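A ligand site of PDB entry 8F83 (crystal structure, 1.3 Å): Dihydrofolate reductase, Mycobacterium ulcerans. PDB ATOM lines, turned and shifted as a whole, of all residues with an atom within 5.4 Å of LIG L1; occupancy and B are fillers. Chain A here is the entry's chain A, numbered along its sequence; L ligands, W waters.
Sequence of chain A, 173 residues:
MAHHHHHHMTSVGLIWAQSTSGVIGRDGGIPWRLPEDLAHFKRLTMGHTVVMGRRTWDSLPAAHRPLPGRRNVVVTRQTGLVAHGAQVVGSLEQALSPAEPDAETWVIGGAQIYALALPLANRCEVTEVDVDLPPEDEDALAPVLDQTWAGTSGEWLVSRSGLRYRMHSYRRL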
ATOM      1  N   ILE A  15       9.354   0.934   6.994  1.00  0.00           N
ATOM      2  CA  ILE A  15       9.492   1.185   5.569  1.00  0.00           C
ATOM      3  C   ILE A  15       8.117   1.400   4.965  1.00  0.00           C
ATOM      4  O   ILE A  15       7.201   0.627   5.242  1.00  0.00           O
ATOM      5  CB  ILE A  15      10.292   0.058   4.881  1.00  0.00           C
ATOM      6  CG1 ILE A  15      10.541   0.375   3.405  1.00  0.00           C
ATOM      7  CG2 ILE A  15       9.621  -1.326   5.110  1.00  0.00           C
ATOM      8  CD1 ILE A  15      11.588  -0.482   2.800  1.00  0.00           C
ATOM      9  N   TRP A  16       7.953   2.503   4.228  1.00  0.00           N
ATOM     10  CA  TRP A  16       6.688   2.830   3.593  1.00  0.00           C
ATOM     11  C   TRP A  16       6.896   3.690   2.373  1.00  0.00           C
ATOM     12  O   TRP A  16       7.942   4.338   2.219  1.00  0.00           O
ATOM     13  CB  TRP A  16       5.740   3.538   4.569  1.00  0.00           C
ATOM     14  CG  TRP A  16       6.004   5.020   4.909  1.00  0.00           C
ATOM     15  CD1 TRP A  16       5.576   6.083   4.200  1.00  0.00           C
ATOM     16  CD2 TRP A  16       6.663   5.552   6.080  1.00  0.00           C
ATOM     17  NE1 TRP A  16       5.912   7.261   4.850  1.00  0.00           N
ATOM     18  CE2 TRP A  16       6.571   6.955   6.003  1.00  0.00           C
ATOM     19  CE3 TRP A  16       7.290   4.972   7.200  1.00  0.00           C
ATOM     20  CZ2 TRP A  16       7.111   7.797   6.986  1.00  0.00           C
ATOM     21  CZ3 TRP A  16       7.820   5.803   8.164  1.00  0.00           C
ATOM     22  CH2 TRP A  16       7.706   7.204   8.063  1.00  0.00           C
ATOM     23  N   ALA A  17       5.872   3.728   1.508  1.00  0.00           N
ATOM     24  CA  ALA A  17       5.818   4.658   0.382  1.00  0.00           C
ATOM     25  C   ALA A  17       4.610   5.562   0.550  1.00  0.00           C
ATOM     26  O   ALA A  17       3.541   5.124   1.003  1.00  0.00           O
ATOM     27  CB  ALA A  17       5.716   3.868  -0.927  1.00  0.00           C
ATOM     28  N   ILE A  30      -3.288   0.622  -2.217  1.00  0.00           N
ATOM     29  CA  ILE A  30      -2.325   1.695  -2.370  1.00  0.00           C
ATOM     30  C   ILE A  30      -2.622   2.416  -3.677  1.00  0.00           C
ATOM     31  O   ILE A  30      -2.591   1.796  -4.749  1.00  0.00           O
ATOM     32  CB  ILE A  30      -0.886   1.167  -2.319  1.00  0.00           C
ATOM     33  CG1 ILE A  30      -0.669   0.505  -0.943  1.00  0.00           C
ATOM     34  CG2 ILE A  30       0.100   2.304  -2.508  1.00  0.00           C
ATOM     35  CD1 ILE A  30       0.619  -0.234  -0.763  1.00  0.00           C
ATOM     36  N   TRP A  32      -1.417   4.213  -6.091  1.00  0.00           N
ATOM     37  CA  TRP A  32      -0.547   4.477  -7.223  1.00  0.00           C
ATOM     38  C   TRP A  32       0.180   3.177  -7.562  1.00  0.00           C
ATOM     39  O   TRP A  32       0.142   2.202  -6.813  1.00  0.00           O
ATOM     40  CB  TRP A  32       0.479   5.611  -6.933  1.00  0.00           C
ATOM     41  CG  TRP A  32       1.362   5.239  -5.781  1.00  0.00           C
ATOM     42  CD1 TRP A  32       2.483   4.446  -5.808  1.00  0.00           C
ATOM     43  CD2 TRP A  32       1.162   5.595  -4.404  1.00  0.00           C
ATOM     44  NE1 TRP A  32       3.000   4.305  -4.530  1.00  0.00           N
ATOM     45  CE2 TRP A  32       2.184   4.982  -3.660  1.00  0.00           C
ATOM     46  CE3 TRP A  32       0.199   6.360  -3.737  1.00  0.00           C
ATOM     47  CZ2 TRP A  32       2.311   5.144  -2.298  1.00  0.00           C
ATOM     48  CZ3 TRP A  32       0.304   6.496  -2.391  1.00  0.00           C
ATOM     49  CH2 TRP A  32       1.341   5.875  -1.680  1.00  0.00           C
ATOM     50  N   ARG A  33       0.876   3.184  -8.701  1.00  0.00           N
ATOM     51  CA  ARG A  33       1.744   2.076  -9.074  1.00  0.00           C
ATOM     52  C   ARG A  33       3.126   2.634  -9.369  1.00  0.00           C
ATOM     53  O   ARG A  33       3.273   3.554 -10.180  1.00  0.00           O
ATOM     54  CB  ARG A  33       1.199   1.306 -10.287  1.00  0.00           C
ATOM     55  CG  ARG A  33       2.068   0.134 -10.743  1.00  0.00           C
ATOM     56  CD  ARG A  33       1.377  -0.698 -11.848  1.00  0.00           C
ATOM     57  NE  ARG A  33       2.340  -1.470 -12.634  1.00  0.00           N
ATOM     58  CZ  ARG A  33       3.106  -0.965 -13.589  1.00  0.00           C
ATOM     59  NH1 ARG A  33       3.073   0.328 -13.885  1.00  0.00           N
ATOM     60  NH2 ARG A  33       3.945  -1.760 -14.249  1.00  0.00           N
ATOM     61  N   LEU A  34       4.122   2.086  -8.702  1.00  0.00           N
ATOM     62  CA  LEU A  34       5.495   2.541  -8.871  1.00  0.00           C
ATOM     63  C   LEU A  34       6.399   1.334  -8.792  1.00  0.00           C
ATOM     64  O   LEU A  34       6.876   0.976  -7.696  1.00  0.00           O
ATOM     65  CB  LEU A  34       5.827   3.568  -7.791  1.00  0.00           C
ATOM     66  CG  LEU A  34       7.205   4.189  -7.965  1.00  0.00           C
ATOM     67  CD1 LEU A  34       7.317   4.769  -9.336  1.00  0.00           C
ATOM     68  CD2 LEU A  34       7.414   5.252  -6.924  1.00  0.00           C
ATOM     69  N   ASP A  37       9.599   1.306  -6.737  1.00  0.00           N
ATOM     70  CA  ASP A  37       9.500   1.253  -5.297  1.00  0.00           C
ATOM     71  C   ASP A  37       9.297  -0.180  -4.821  1.00  0.00           C
ATOM     72  O   ASP A  37       9.800  -0.555  -3.755  1.00  0.00           O
ATOM     73  CB  ASP A  37       8.347   2.124  -4.804  1.00  0.00           C
ATOM     74  CG  ASP A  37       8.089   1.907  -3.327  1.00  0.00           C
ATOM     75  OD1 ASP A  37       8.963   2.244  -2.504  1.00  0.00           O
ATOM     76  OD2 ASP A  37       7.015   1.351  -2.976  1.00  0.00           O
ATOM     77  N   LEU A  38       8.550  -0.999  -5.575  1.00  0.00           N
ATOM     78  CA  LEU A  38       8.421  -2.396  -5.180  1.00  0.00           C
ATOM     79  C   LEU A  38       9.775  -3.098  -5.195  1.00  0.00           C
ATOM     80  O   LEU A  38      10.103  -3.848  -4.275  1.00  0.00           O
ATOM     81  CB  LEU A  38       7.400  -3.099  -6.082  1.00  0.00           C
ATOM     82  CG  LEU A  38       7.217  -4.597  -5.875  1.00  0.00           C
ATOM     83  CD1 LEU A  38       7.017  -4.962  -4.377  1.00  0.00           C
ATOM     84  CD2 LEU A  38       6.049  -5.104  -6.701  1.00  0.00           C
ATOM     85  N   HIS A  40      12.709  -1.646  -4.707  1.00  0.00           N
ATOM     86  CA  HIS A  40      13.399  -1.099  -3.538  1.00  0.00           C
ATOM     87  C   HIS A  40      12.946  -1.814  -2.277  1.00  0.00           C
ATOM     88  O   HIS A  40      13.772  -2.213  -1.437  1.00  0.00           O
ATOM     89  CB  HIS A  40      13.100   0.414  -3.499  1.00  0.00           C
ATOM     90  CG  HIS A  40      13.427   1.092  -2.213  1.00  0.00           C
ATOM     91  ND1 HIS A  40      14.715   1.388  -1.835  1.00  0.00           N
ATOM     92  CD2 HIS A  40      12.618   1.625  -1.269  1.00  0.00           C
ATOM     93  CE1 HIS A  40      14.691   2.061  -0.699  1.00  0.00           C
ATOM     94  NE2 HIS A  40      13.434   2.201  -0.332  1.00  0.00           N
ATOM     95  N   PHE A  41      11.620  -1.961  -2.101  1.00  0.00           N
ATOM     96  CA  PHE A  41      11.062  -2.615  -0.931  1.00  0.00           C
ATOM     97  C   PHE A  41      11.556  -4.058  -0.812  1.00  0.00           C
ATOM     98  O   PHE A  41      11.975  -4.506   0.265  1.00  0.00           O
ATOM     99  CB  PHE A  41       9.526  -2.566  -0.994  1.00  0.00           C
ATOM    100  CG  PHE A  41       8.854  -3.371   0.061  1.00  0.00           C
ATOM    101  CD1 PHE A  41       8.752  -2.879   1.361  1.00  0.00           C
ATOM    102  CD2 PHE A  41       8.323  -4.645  -0.226  1.00  0.00           C
ATOM    103  CE1 PHE A  41       8.154  -3.626   2.372  1.00  0.00           C
ATOM    104  CE2 PHE A  41       7.694  -5.386   0.758  1.00  0.00           C
ATOM    105  CZ  PHE A  41       7.656  -4.895   2.056  1.00  0.00           C
ATOM    106  N   LYS A  42      11.565  -4.777  -1.926  1.00  0.00           N
ATOM    107  CA  LYS A  42      12.083  -6.155  -1.925  1.00  0.00           C
ATOM    108  C   LYS A  42      13.559  -6.207  -1.536  1.00  0.00           C
ATOM    109  O   LYS A  42      13.970  -7.025  -0.712  1.00  0.00           O
ATOM    110  CB  LYS A  42      11.894  -6.773  -3.304  1.00  0.00           C
ATOM    111  CG  LYS A  42      10.489  -7.213  -3.640  1.00  0.00           C
ATOM    112  CD  LYS A  42      10.549  -8.041  -4.945  1.00  0.00           C
ATOM    113  CE  LYS A  42       9.232  -8.188  -5.581  1.00  0.00           C
ATOM    114  NZ  LYS A  42       9.394  -8.672  -6.961  1.00  0.00           N
ATOM    115  N   THR A  45      14.019  -5.617   2.256  1.00  0.00           N
ATOM    116  CA  THR A  45      13.401  -6.551   3.196  1.00  0.00           C
ATOM    117  C   THR A  45      13.771  -8.020   2.960  1.00  0.00           C
ATOM    118  O   THR A  45      13.521  -8.847   3.849  1.00  0.00           O
ATOM    119  CB  THR A  45      11.865  -6.401   3.211  1.00  0.00           C
ATOM    120  OG1 THR A  45      11.308  -6.676   1.889  1.00  0.00           O
ATOM    121  CG2 THR A  45      11.394  -5.034   3.685  1.00  0.00           C
ATOM    122  N   THR A  56      -3.279  -4.840   6.373  1.00  0.00           N
ATOM    123  CA  THR A  56      -2.273  -4.934   5.305  1.00  0.00           C
ATOM    124  C   THR A  56      -2.121  -6.375   4.814  1.00  0.00           C
ATOM    125  O   THR A  56      -2.092  -6.619   3.616  1.00  0.00           O
ATOM    126  CB  THR A  56      -0.937  -4.356   5.790  1.00  0.00           C
ATOM    127  OG1 THR A  56      -1.088  -2.951   6.016  1.00  0.00           O
ATOM    128  CG2 THR A  56       0.215  -4.615   4.794  1.00  0.00           C
ATOM    129  N   LEU A  60      -2.941  -7.682   0.673  1.00  0.00           N
ATOM    130  CA  LEU A  60      -1.961  -8.149  -0.287  1.00  0.00           C
ATOM    131  C   LEU A  60      -2.669  -8.882  -1.421  1.00  0.00           C
ATOM    132  O   LEU A  60      -3.573  -9.709  -1.162  1.00  0.00           O
ATOM    133  CB  LEU A  60      -0.962  -9.112   0.369  1.00  0.00           C
ATOM    134  CG  LEU A  60      -0.080  -8.460   1.435  1.00  0.00           C
ATOM    135  CD1 LEU A  60       0.711  -9.578   2.158  1.00  0.00           C
ATOM    136  CD2 LEU A  60       0.855  -7.442   0.772  1.00  0.00           C
ATOM    137  N   PRO A  61      -2.293  -8.630  -2.668  1.00  0.00           N
ATOM    138  CA  PRO A  61      -2.773  -9.506  -3.739  1.00  0.00           C
ATOM    139  C   PRO A  61      -2.311 -10.933  -3.470  1.00  0.00           C
ATOM    140  O   PRO A  61      -1.282 -11.159  -2.832  1.00  0.00           O
ATOM    141  CB  PRO A  61      -2.104  -8.929  -5.000  1.00  0.00           C
ATOM    142  CG  PRO A  61      -1.740  -7.510  -4.636  1.00  0.00           C
ATOM    143  CD  PRO A  61      -1.407  -7.564  -3.164  1.00  0.00           C
ATOM    144  N   HIS A  64       1.196 -12.206  -3.808  1.00  0.00           N
ATOM    145  CA  HIS A  64       2.175 -11.593  -2.923  1.00  0.00           C
ATOM    146  C   HIS A  64       1.966 -11.932  -1.450  1.00  0.00           C
ATOM    147  O   HIS A  64       2.629 -11.319  -0.593  1.00  0.00           O
ATOM    148  CB  HIS A  64       2.151 -10.091  -3.150  1.00  0.00           C
ATOM    149  CG  HIS A  64       2.493  -9.708  -4.551  1.00  0.00           C
ATOM    150  ND1 HIS A  64       3.759  -9.834  -5.072  1.00  0.00           N
ATOM    151  CD2 HIS A  64       1.726  -9.220  -5.560  1.00  0.00           C
ATOM    152  CE1 HIS A  64       3.769  -9.446  -6.338  1.00  0.00           C
ATOM    153  NE2 HIS A  64       2.544  -9.063  -6.658  1.00  0.00           N
ATOM    154  N   LEU A  67       4.709 -12.586   1.652  1.00  0.00           N
ATOM    155  CA  LEU A  67       5.816 -12.012   0.898  1.00  0.00           C
ATOM    156  C   LEU A  67       6.910 -13.071   0.791  1.00  0.00           C
ATOM    157  O   LEU A  67       7.444 -13.496   1.817  1.00  0.00           O
ATOM    158  CB  LEU A  67       6.336 -10.758   1.597  1.00  0.00           C
ATOM    159  CG  LEU A  67       5.281  -9.659   1.679  1.00  0.00           C
ATOM    160  CD1 LEU A  67       5.843  -8.421   2.350  1.00  0.00           C
ATOM    161  CD2 LEU A  67       4.817  -9.322   0.314  1.00  0.00           C
ATOM    162  N   PRO A  68       7.293 -13.497  -0.402  1.00  0.00           N
ATOM    163  CA  PRO A  68       8.233 -14.627  -0.505  1.00  0.00           C
ATOM    164  C   PRO A  68       9.624 -14.242  -0.030  1.00  0.00           C
ATOM    165  O   PRO A  68      10.079 -13.113  -0.195  1.00  0.00           O
ATOM    166  CB  PRO A  68       8.230 -14.967  -1.996  1.00  0.00           C
ATOM    167  CG  PRO A  68       7.855 -13.697  -2.661  1.00  0.00           C
ATOM    168  CD  PRO A  68       6.847 -13.031  -1.729  1.00  0.00           C
ATOM    169  N   ARG A  70      10.716 -13.965   3.033  1.00  0.00           N
ATOM    170  CA  ARG A  70      10.739 -13.192   4.243  1.00  0.00           C
ATOM    171  C   ARG A  70       9.837 -13.905   5.238  1.00  0.00           C
ATOM    172  O   ARG A  70       8.901 -14.601   4.838  1.00  0.00           O
ATOM    173  CB  ARG A  70      10.178 -11.792   3.968  1.00  0.00           C
ATOM    174  CG  ARG A  70      11.246 -10.883   3.348  1.00  0.00           C
ATOM    175  CD  ARG A  70      10.713  -9.890   2.323  1.00  0.00           C
ATOM    176  NE  ARG A  70      10.179 -10.486   1.102  1.00  0.00           N
ATOM    177  CZ  ARG A  70       9.562  -9.787   0.152  1.00  0.00           C
ATOM    178  NH1 ARG A  70       9.392  -8.481   0.253  1.00  0.00           N
ATOM    179  NH2 ARG A  70       9.055 -10.446  -0.886  1.00  0.00           N
ATOM    180  N   VAL A 107       9.038  -3.162   9.792  1.00  0.00           N
ATOM    181  CA  VAL A 107       7.619  -2.923   9.944  1.00  0.00           C
ATOM    182  C   VAL A 107       7.111  -2.309   8.634  1.00  0.00           C
ATOM    183  O   VAL A 107       7.612  -1.239   8.208  1.00  0.00           O
ATOM    184  CB  VAL A 107       7.325  -2.034  11.161  1.00  0.00           C
ATOM    185  CG1 VAL A 107       5.872  -1.704  11.209  1.00  0.00           C
ATOM    186  CG2 VAL A 107       7.809  -2.707  12.474  1.00  0.00           C
ATOM    187  N   ILE A 108       6.183  -2.993   7.974  1.00  0.00           N
ATOM    188  CA  ILE A 108       5.872  -2.695   6.584  1.00  0.00           C
ATOM    189  C   ILE A 108       4.453  -2.183   6.390  1.00  0.00           C
ATOM    190  O   ILE A 108       3.968  -2.082   5.249  1.00  0.00           O
ATOM    191  CB  ILE A 108       6.135  -3.913   5.661  1.00  0.00           C
ATOM    192  CG1 ILE A 108       5.093  -5.008   5.974  1.00  0.00           C
ATOM    193  CG2 ILE A 108       7.554  -4.423   5.810  1.00  0.00           C
ATOM    194  CD1 ILE A 108       5.053  -6.086   4.855  1.00  0.00           C
ATOM    195  N   GLY A 109       3.769  -1.844   7.481  1.00  0.00           N
ATOM    196  CA  GLY A 109       2.483  -1.169   7.452  1.00  0.00           C
ATOM    197  C   GLY A 109       1.403  -1.950   8.161  1.00  0.00           C
ATOM    198  O   GLY A 109       1.614  -3.056   8.648  1.00  0.00           O
ATOM    199  N   TYR A 114       2.260   1.222  12.027  1.00  0.00           N
ATOM    200  CA  TYR A 114       3.343   2.237  12.063  1.00  0.00           C
ATOM    201  C   TYR A 114       3.278   3.040  13.354  1.00  0.00           C
ATOM    202  O   TYR A 114       4.298   3.320  13.976  1.00  0.00           O
ATOM    203  CB  TYR A 114       3.296   3.209  10.870  1.00  0.00           C
ATOM    204  CG  TYR A 114       3.678   2.608   9.529  1.00  0.00           C
ATOM    205  CD1 TYR A 114       4.761   1.722   9.389  1.00  0.00           C
ATOM    206  CD2 TYR A 114       2.930   2.912   8.391  1.00  0.00           C
ATOM    207  CE1 TYR A 114       5.096   1.171   8.131  1.00  0.00           C
ATOM    208  CE2 TYR A 114       3.252   2.337   7.148  1.00  0.00           C
ATOM    209  CZ  TYR A 114       4.329   1.498   7.021  1.00  0.00           C
ATOM    210  OH  TYR A 114       4.574   0.949   5.792  1.00  0.00           O
ATOM    211  N   GLU A 125      12.657   4.154   6.330  1.00  0.00           N
ATOM    212  CA  GLU A 125      12.999   4.201   4.913  1.00  0.00           C
ATOM    213  C   GLU A 125      11.734   4.559   4.155  1.00  0.00           C
ATOM    214  O   GLU A 125      10.777   3.776   4.137  1.00  0.00           O
ATOM    215  CB  GLU A 125      13.558   2.855   4.439  1.00  0.00           C
ATOM    216  CG  GLU A 125      14.894   2.544   5.059  1.00  0.00           C
ATOM    217  CD  GLU A 125      15.963   3.501   4.564  1.00  0.00           C
ATOM    218  OE1 GLU A 125      15.748   4.150   3.524  1.00  0.00           O
ATOM    219  OE2 GLU A 125      17.003   3.621   5.239  1.00  0.00           O
ATOM    220  N   THR A 127       9.754   6.092   0.710  1.00  0.00           N
ATOM    221  CA  THR A 127       9.673   6.491  -0.689  1.00  0.00           C
ATOM    222  C   THR A 127       8.601   7.547  -0.805  1.00  0.00           C
ATOM    223  O   THR A 127       7.451   7.311  -0.431  1.00  0.00           O
ATOM    224  CB  THR A 127       9.379   5.305  -1.612  1.00  0.00           C
ATOM    225  OG1 THR A 127      10.349   4.281  -1.396  1.00  0.00           O
ATOM    226  CG2 THR A 127       9.377   5.776  -3.089  1.00  0.00           C
HETATM  227  C1  LIG L   1       7.338   0.545   0.442  1.00  0.00           C
HETATM  228  C2  LIG L   1       6.186  -0.684   1.974  1.00  0.00           C
HETATM  229  C3  LIG L   1       5.312  -1.134   0.942  1.00  0.00           C
HETATM  230  C4  LIG L   1       4.492  -3.327   1.619  1.00  0.00           C
HETATM  231  C5  LIG L   1       3.179  -4.034   1.822  1.00  0.00           C
HETATM  232  C6  LIG L   1       2.418  -4.240   0.525  1.00  0.00           C
HETATM  233  C7  LIG L   1       2.724  -5.370  -1.599  1.00  0.00           C
HETATM  234  C8  LIG L   1       2.973  -1.414  -3.683  1.00  0.00           C
HETATM  235  C9  LIG L   1       2.033  -1.641  -4.822  1.00  0.00           C
HETATM  236  C10 LIG L   1       3.246  -0.137  -3.246  1.00  0.00           C
HETATM  237  C11 LIG L   1       4.074   0.059  -2.166  1.00  0.00           C
HETATM  238  N1  LIG L   1       7.218   0.143   1.711  1.00  0.00           N
HETATM  239  O1  LIG L   1       4.232  -1.957   1.222  1.00  0.00           O
HETATM  240  O2  LIG L   1       7.319  -9.323  -2.643  1.00  0.00           O
HETATM  241  C12 LIG L   1       1.874  -5.919  -4.174  1.00  0.00           C
HETATM  242  C13 LIG L   1       3.095  -6.393  -3.718  1.00  0.00           C
HETATM  243  C14 LIG L   1       3.557  -6.141  -2.426  1.00  0.00           C
HETATM  244  C15 LIG L   1       4.913  -6.636  -1.935  1.00  0.00           C
HETATM  245  C16 LIG L   1       5.480  -7.829  -2.688  1.00  0.00           C
HETATM  246  C17 LIG L   1       6.884  -8.221  -2.252  1.00  0.00           C
HETATM  247  C18 LIG L   1       5.523  -0.664  -0.343  1.00  0.00           C
HETATM  248  C19 LIG L   1       4.688  -1.015  -1.519  1.00  0.00           C
HETATM  249  C20 LIG L   1       4.329  -2.300  -1.908  1.00  0.00           C
HETATM  250  C21 LIG L   1       3.514  -2.500  -3.008  1.00  0.00           C
HETATM  251  C22 LIG L   1       1.501  -4.905  -2.045  1.00  0.00           C
HETATM  252  C23 LIG L   1       1.080  -5.179  -3.340  1.00  0.00           C
HETATM  253  F1  LIG L   1       0.843  -2.021  -4.370  1.00  0.00           F
HETATM  254  F2  LIG L   1       2.410  -2.582  -5.651  1.00  0.00           F
HETATM  255  F3  LIG L   1       1.796  -0.549  -5.577  1.00  0.00           F
HETATM  256  N2  LIG L   1       8.378   1.357   0.147  1.00  0.00           N
HETATM  257  N3  LIG L   1       5.988  -1.027   3.276  1.00  0.00           N
HETATM  258  N4  LIG L   1       6.535   0.187  -0.579  1.00  0.00           N
HETATM  259  O3  LIG L   1       3.200  -5.112  -0.338  1.00  0.00           O
HETATM  260  O4  LIG L   1       7.553  -7.453  -1.532  1.00  0.00           O
HETATM  261  P1  LG2 L   2      -3.025  -2.054   9.472  1.00  0.00           P
HETATM  262  O1  LG2 L   2      -2.128  -1.240  10.361  1.00  0.00           O
HETATM  263  O2  LG2 L   2      -2.393  -2.787   8.335  1.00  0.00           O
HETATM  264  O3  LG2 L   2      -3.824  -3.171  10.318  1.00  0.00           O
HETATM  265  C1  LG2 L   2      -4.743  -2.832  11.382  1.00  0.00           C
HETATM  266  C2  LG2 L   2      -5.038  -4.095  12.143  1.00  0.00           C
HETATM  267  O4  LG2 L   2      -3.888  -4.481  12.939  1.00  0.00           O
HETATM  268  C3  LG2 L   2      -6.196  -4.026  13.153  1.00  0.00           C
HETATM  269  O5  LG2 L   2      -7.429  -4.116  12.444  1.00  0.00           O
HETATM  270  C4  LG2 L   2      -5.842  -5.192  14.073  1.00  0.00           C
HETATM  271  O6  LG2 L   2      -6.066  -6.460  13.435  1.00  0.00           O
HETATM  272  C5  LG2 L   2      -4.326  -5.036  14.151  1.00  0.00           C
HETATM  273  N1  LG2 L   2      -3.876  -4.227  15.274  1.00  0.00           N
HETATM  274  C6  LG2 L   2      -3.726  -2.869  15.317  1.00  0.00           C
HETATM  275  N2  LG2 L   2      -3.307  -2.443  16.490  1.00  0.00           N
HETATM  276  C7  LG2 L   2      -3.158  -3.594  17.251  1.00  0.00           C
HETATM  277  C8  LG2 L   2      -2.716  -3.807  18.570  1.00  0.00           C
HETATM  278  N3  LG2 L   2      -2.351  -2.836  19.410  1.00  0.00           N
HETATM  279  N4  LG2 L   2      -2.668  -5.098  19.011  1.00  0.00           N
HETATM  280  C9  LG2 L   2      -3.040  -6.076  18.173  1.00  0.00           C
HETATM  281  N5  LG2 L   2      -3.484  -5.989  16.913  1.00  0.00           N
HETATM  282  C10 LG2 L   2      -3.501  -4.703  16.500  1.00  0.00           C
HETATM  283  O7  LG2 L   2      -4.239  -1.175   8.924  1.00  0.00           O
HETATM  284  P2  LG2 L   2      -4.397   0.296   8.335  1.00  0.00           P
HETATM  285  O8  LG2 L   2      -3.818   1.314   9.260  1.00  0.00           O
HETATM  286  O9  LG2 L   2      -5.821   0.460   7.926  1.00  0.00           O
HETATM  287  O10 LG2 L   2      -3.450   0.215   7.047  1.00  0.00           O
HETATM  288  C11 LG2 L   2      -3.962  -0.482   5.864  1.00  0.00           C
HETATM  289  C12 LG2 L   2      -3.801   0.438   4.670  1.00  0.00           C
HETATM  290  O11 LG2 L   2      -2.404   0.788   4.526  1.00  0.00           O
HETATM  291  C13 LG2 L   2      -4.186  -0.208   3.330  1.00  0.00           C
HETATM  292  O12 LG2 L   2      -4.739   0.778   2.456  1.00  0.00           O
HETATM  293  C14 LG2 L   2      -2.851  -0.703   2.780  1.00  0.00           C
HETATM  294  O13 LG2 L   2      -2.961  -0.827   1.369  1.00  0.00           O
HETATM  295  C15 LG2 L   2      -1.998   0.488   3.193  1.00  0.00           C
HETATM  296  N6  LG2 L   2      -0.539   0.243   3.228  1.00  0.00           N
HETATM  297  C16 LG2 L   2       0.294   1.109   2.572  1.00  0.00           C
HETATM  298  C17 LG2 L   2       1.672   0.915   2.604  1.00  0.00           C
HETATM  299  C18 LG2 L   2       2.577   1.877   1.890  1.00  0.00           C
HETATM  300  O14 LG2 L   2       3.801   1.763   2.039  1.00  0.00           O
HETATM  301  N7  LG2 L   2       2.017   2.794   1.124  1.00  0.00           N
HETATM  302  C19 LG2 L   2       2.192  -0.152   3.330  1.00  0.00           C
HETATM  303  C20 LG2 L   2       1.331  -1.023   3.978  1.00  0.00           C
HETATM  304  C21 LG2 L   2      -0.023  -0.827   3.932  1.00  0.00           C
HETATM  305  P3  LG2 L   2      -7.479  -7.196  13.760  1.00  0.00           P
HETATM  306  O15 LG2 L   2      -7.512  -7.409  15.248  1.00  0.00           O
HETATM  307  O16 LG2 L   2      -8.585  -6.321  13.231  1.00  0.00           O
HETATM  308  O17 LG2 L   2      -7.322  -8.478  12.957  1.00  0.00           O
HETATM  309  O   HOH W   1       4.942   2.293  -4.525  1.00  0.00           O
HETATM  310  O   HOH W   2      -1.242  -0.399  -6.403  1.00  0.00           O
HETATM  311  O   HOH W   3       5.969 -11.019  -4.035  1.00  0.00           O
HETATM  312  O   HOH W   4       1.762  -3.596  -8.865  1.00  0.00           O
HETATM  313  O   HOH W   5      10.771   2.928   1.170  1.00  0.00           O
HETATM  314  O   HOH W   6       4.741  -0.016  -6.440  1.00  0.00           O
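OG1 of Thr 56 lies within hydrogen-bond range of O2 of LG2 L2 (2.7 Å).
OH of Tyr 114 is in hydrogen-bond range of N3 of LIG L1 (3.5 Å).
The backbone carbonyl oxygen of Ile 15 is in hydrogen-bond range of a nitrogen (N3) of LIG L1 (2.8 Å).
N of Ala 17 lies within hydrogen-bond range of O14 of LG2 L2, 2.9 Å away.
O of Ala 17 is in hydrogen-bond range of N7 of LG2 L2 (2.8 Å).
The guanidinium group (NH2) of Arg 70 lies within salt-bridge range of an oxygen (O2) of LIG L1, at 2.7 Å.
The backbone NH (N) of Thr 56 sits at hydrogen-bond distance from an oxygen (O2) of LG2 L2 (3.0 Å).
OD2 of Asp 37 lies within hydrogen-bond range of N4 of LIG L1 (2.7 Å).
O of Ile 108 is in hydrogen-bond range of N3 of LIG L1, 3.0 Å away.
The backbone carbonyl oxygen (O) of Ile 15 is in hydrogen-bond range of the side-chain hydroxyl (OH) of Tyr 114, 2.7 Å away.
The guanidinium group (NE) of Arg 70 sits at hydrogen-bond distance from the backbone carbonyl oxygen (O) of Pro 68 (2.9 Å).
O of Val 107 lies within hydrogen-bond range of N of Ile 15, 3.0 Å away.
O of Trp 16 lies within hydrogen-bond range of N of Thr 127 (2.9 Å).
The backbone NH of Gly 109 sits close to the side-chain hydroxyl of Tyr 114 (3.4 Å).
The side-chain carboxylate (OD1) of Asp 37 is in hydrogen-bond range of the side-chain hydroxyl (OG1) of Thr 127, at 2.7 Å.
The backbone NH (N) of Trp 16 lies within hydrogen-bond range of the backbone carbonyl oxygen (O) of Glu 125 (3.1 Å).
NH1 of Arg 70 is in hydrogen-bond range of OG1 of Thr 45 (3.1 Å).
The backbone carbonyl oxygen (O) of Trp 32 sits close to a fluorine (F3) of LIG L1, at 3.4 Å.
Trp 16 touches LIG L1.
N of Ala 17 touches C1 of LIG L1, at 3.7 Å.
Ile 30 touches LIG L1.
Leu 38 touches LIG L1.
CE2 of Phe 41 touches O4 of LIG L1 (3.1 Å).
Lys 42 touches LIG L1.
Leu 60 touches LIG L1 (CD2 to O3, 3.5 Å).
Pro 61 touches LIG L1.
His 64 touches LIG L1 (CG to C13, 3.5 Å).
CD2 of Leu 67 touches C16 of LIG L1 (3.4 Å).
Pro 68 touches LIG L1 (CD to O2, 3.8 Å).
Thr 127 touches LIG L1.
18 residues have an atom within 4 Å of LIG L1: Ile 15, Trp 16, Ala 17, Ile 30, Trp 32, Asp 37, Leu 38, Phe 41, Lys 42, Leu 60, Pro 61, His 64, Leu 67, Pro 68, Arg 70, Ile 108, Tyr 114 and Thr 127.
Water W3 lies within hydrogen-bond range of an oxygen (O2) of LIG L1 and a ring nitrogen (ND1) of His 64.
Water W5 lies within hydrogen-bond range of the side-chain hydroxyl of Thr 127, a nitrogen (N2) of LIG L1, the backbone carbonyl oxygen of Glu 125, a ring nitrogen (NE2) of His 40 and the backbone carbonyl oxygen of Trp 16.
Water W1 lies within hydrogen-bond range of OD2 of Asp 37 (2.8 Å) and NE1 of Trp 32 (2.8 Å).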
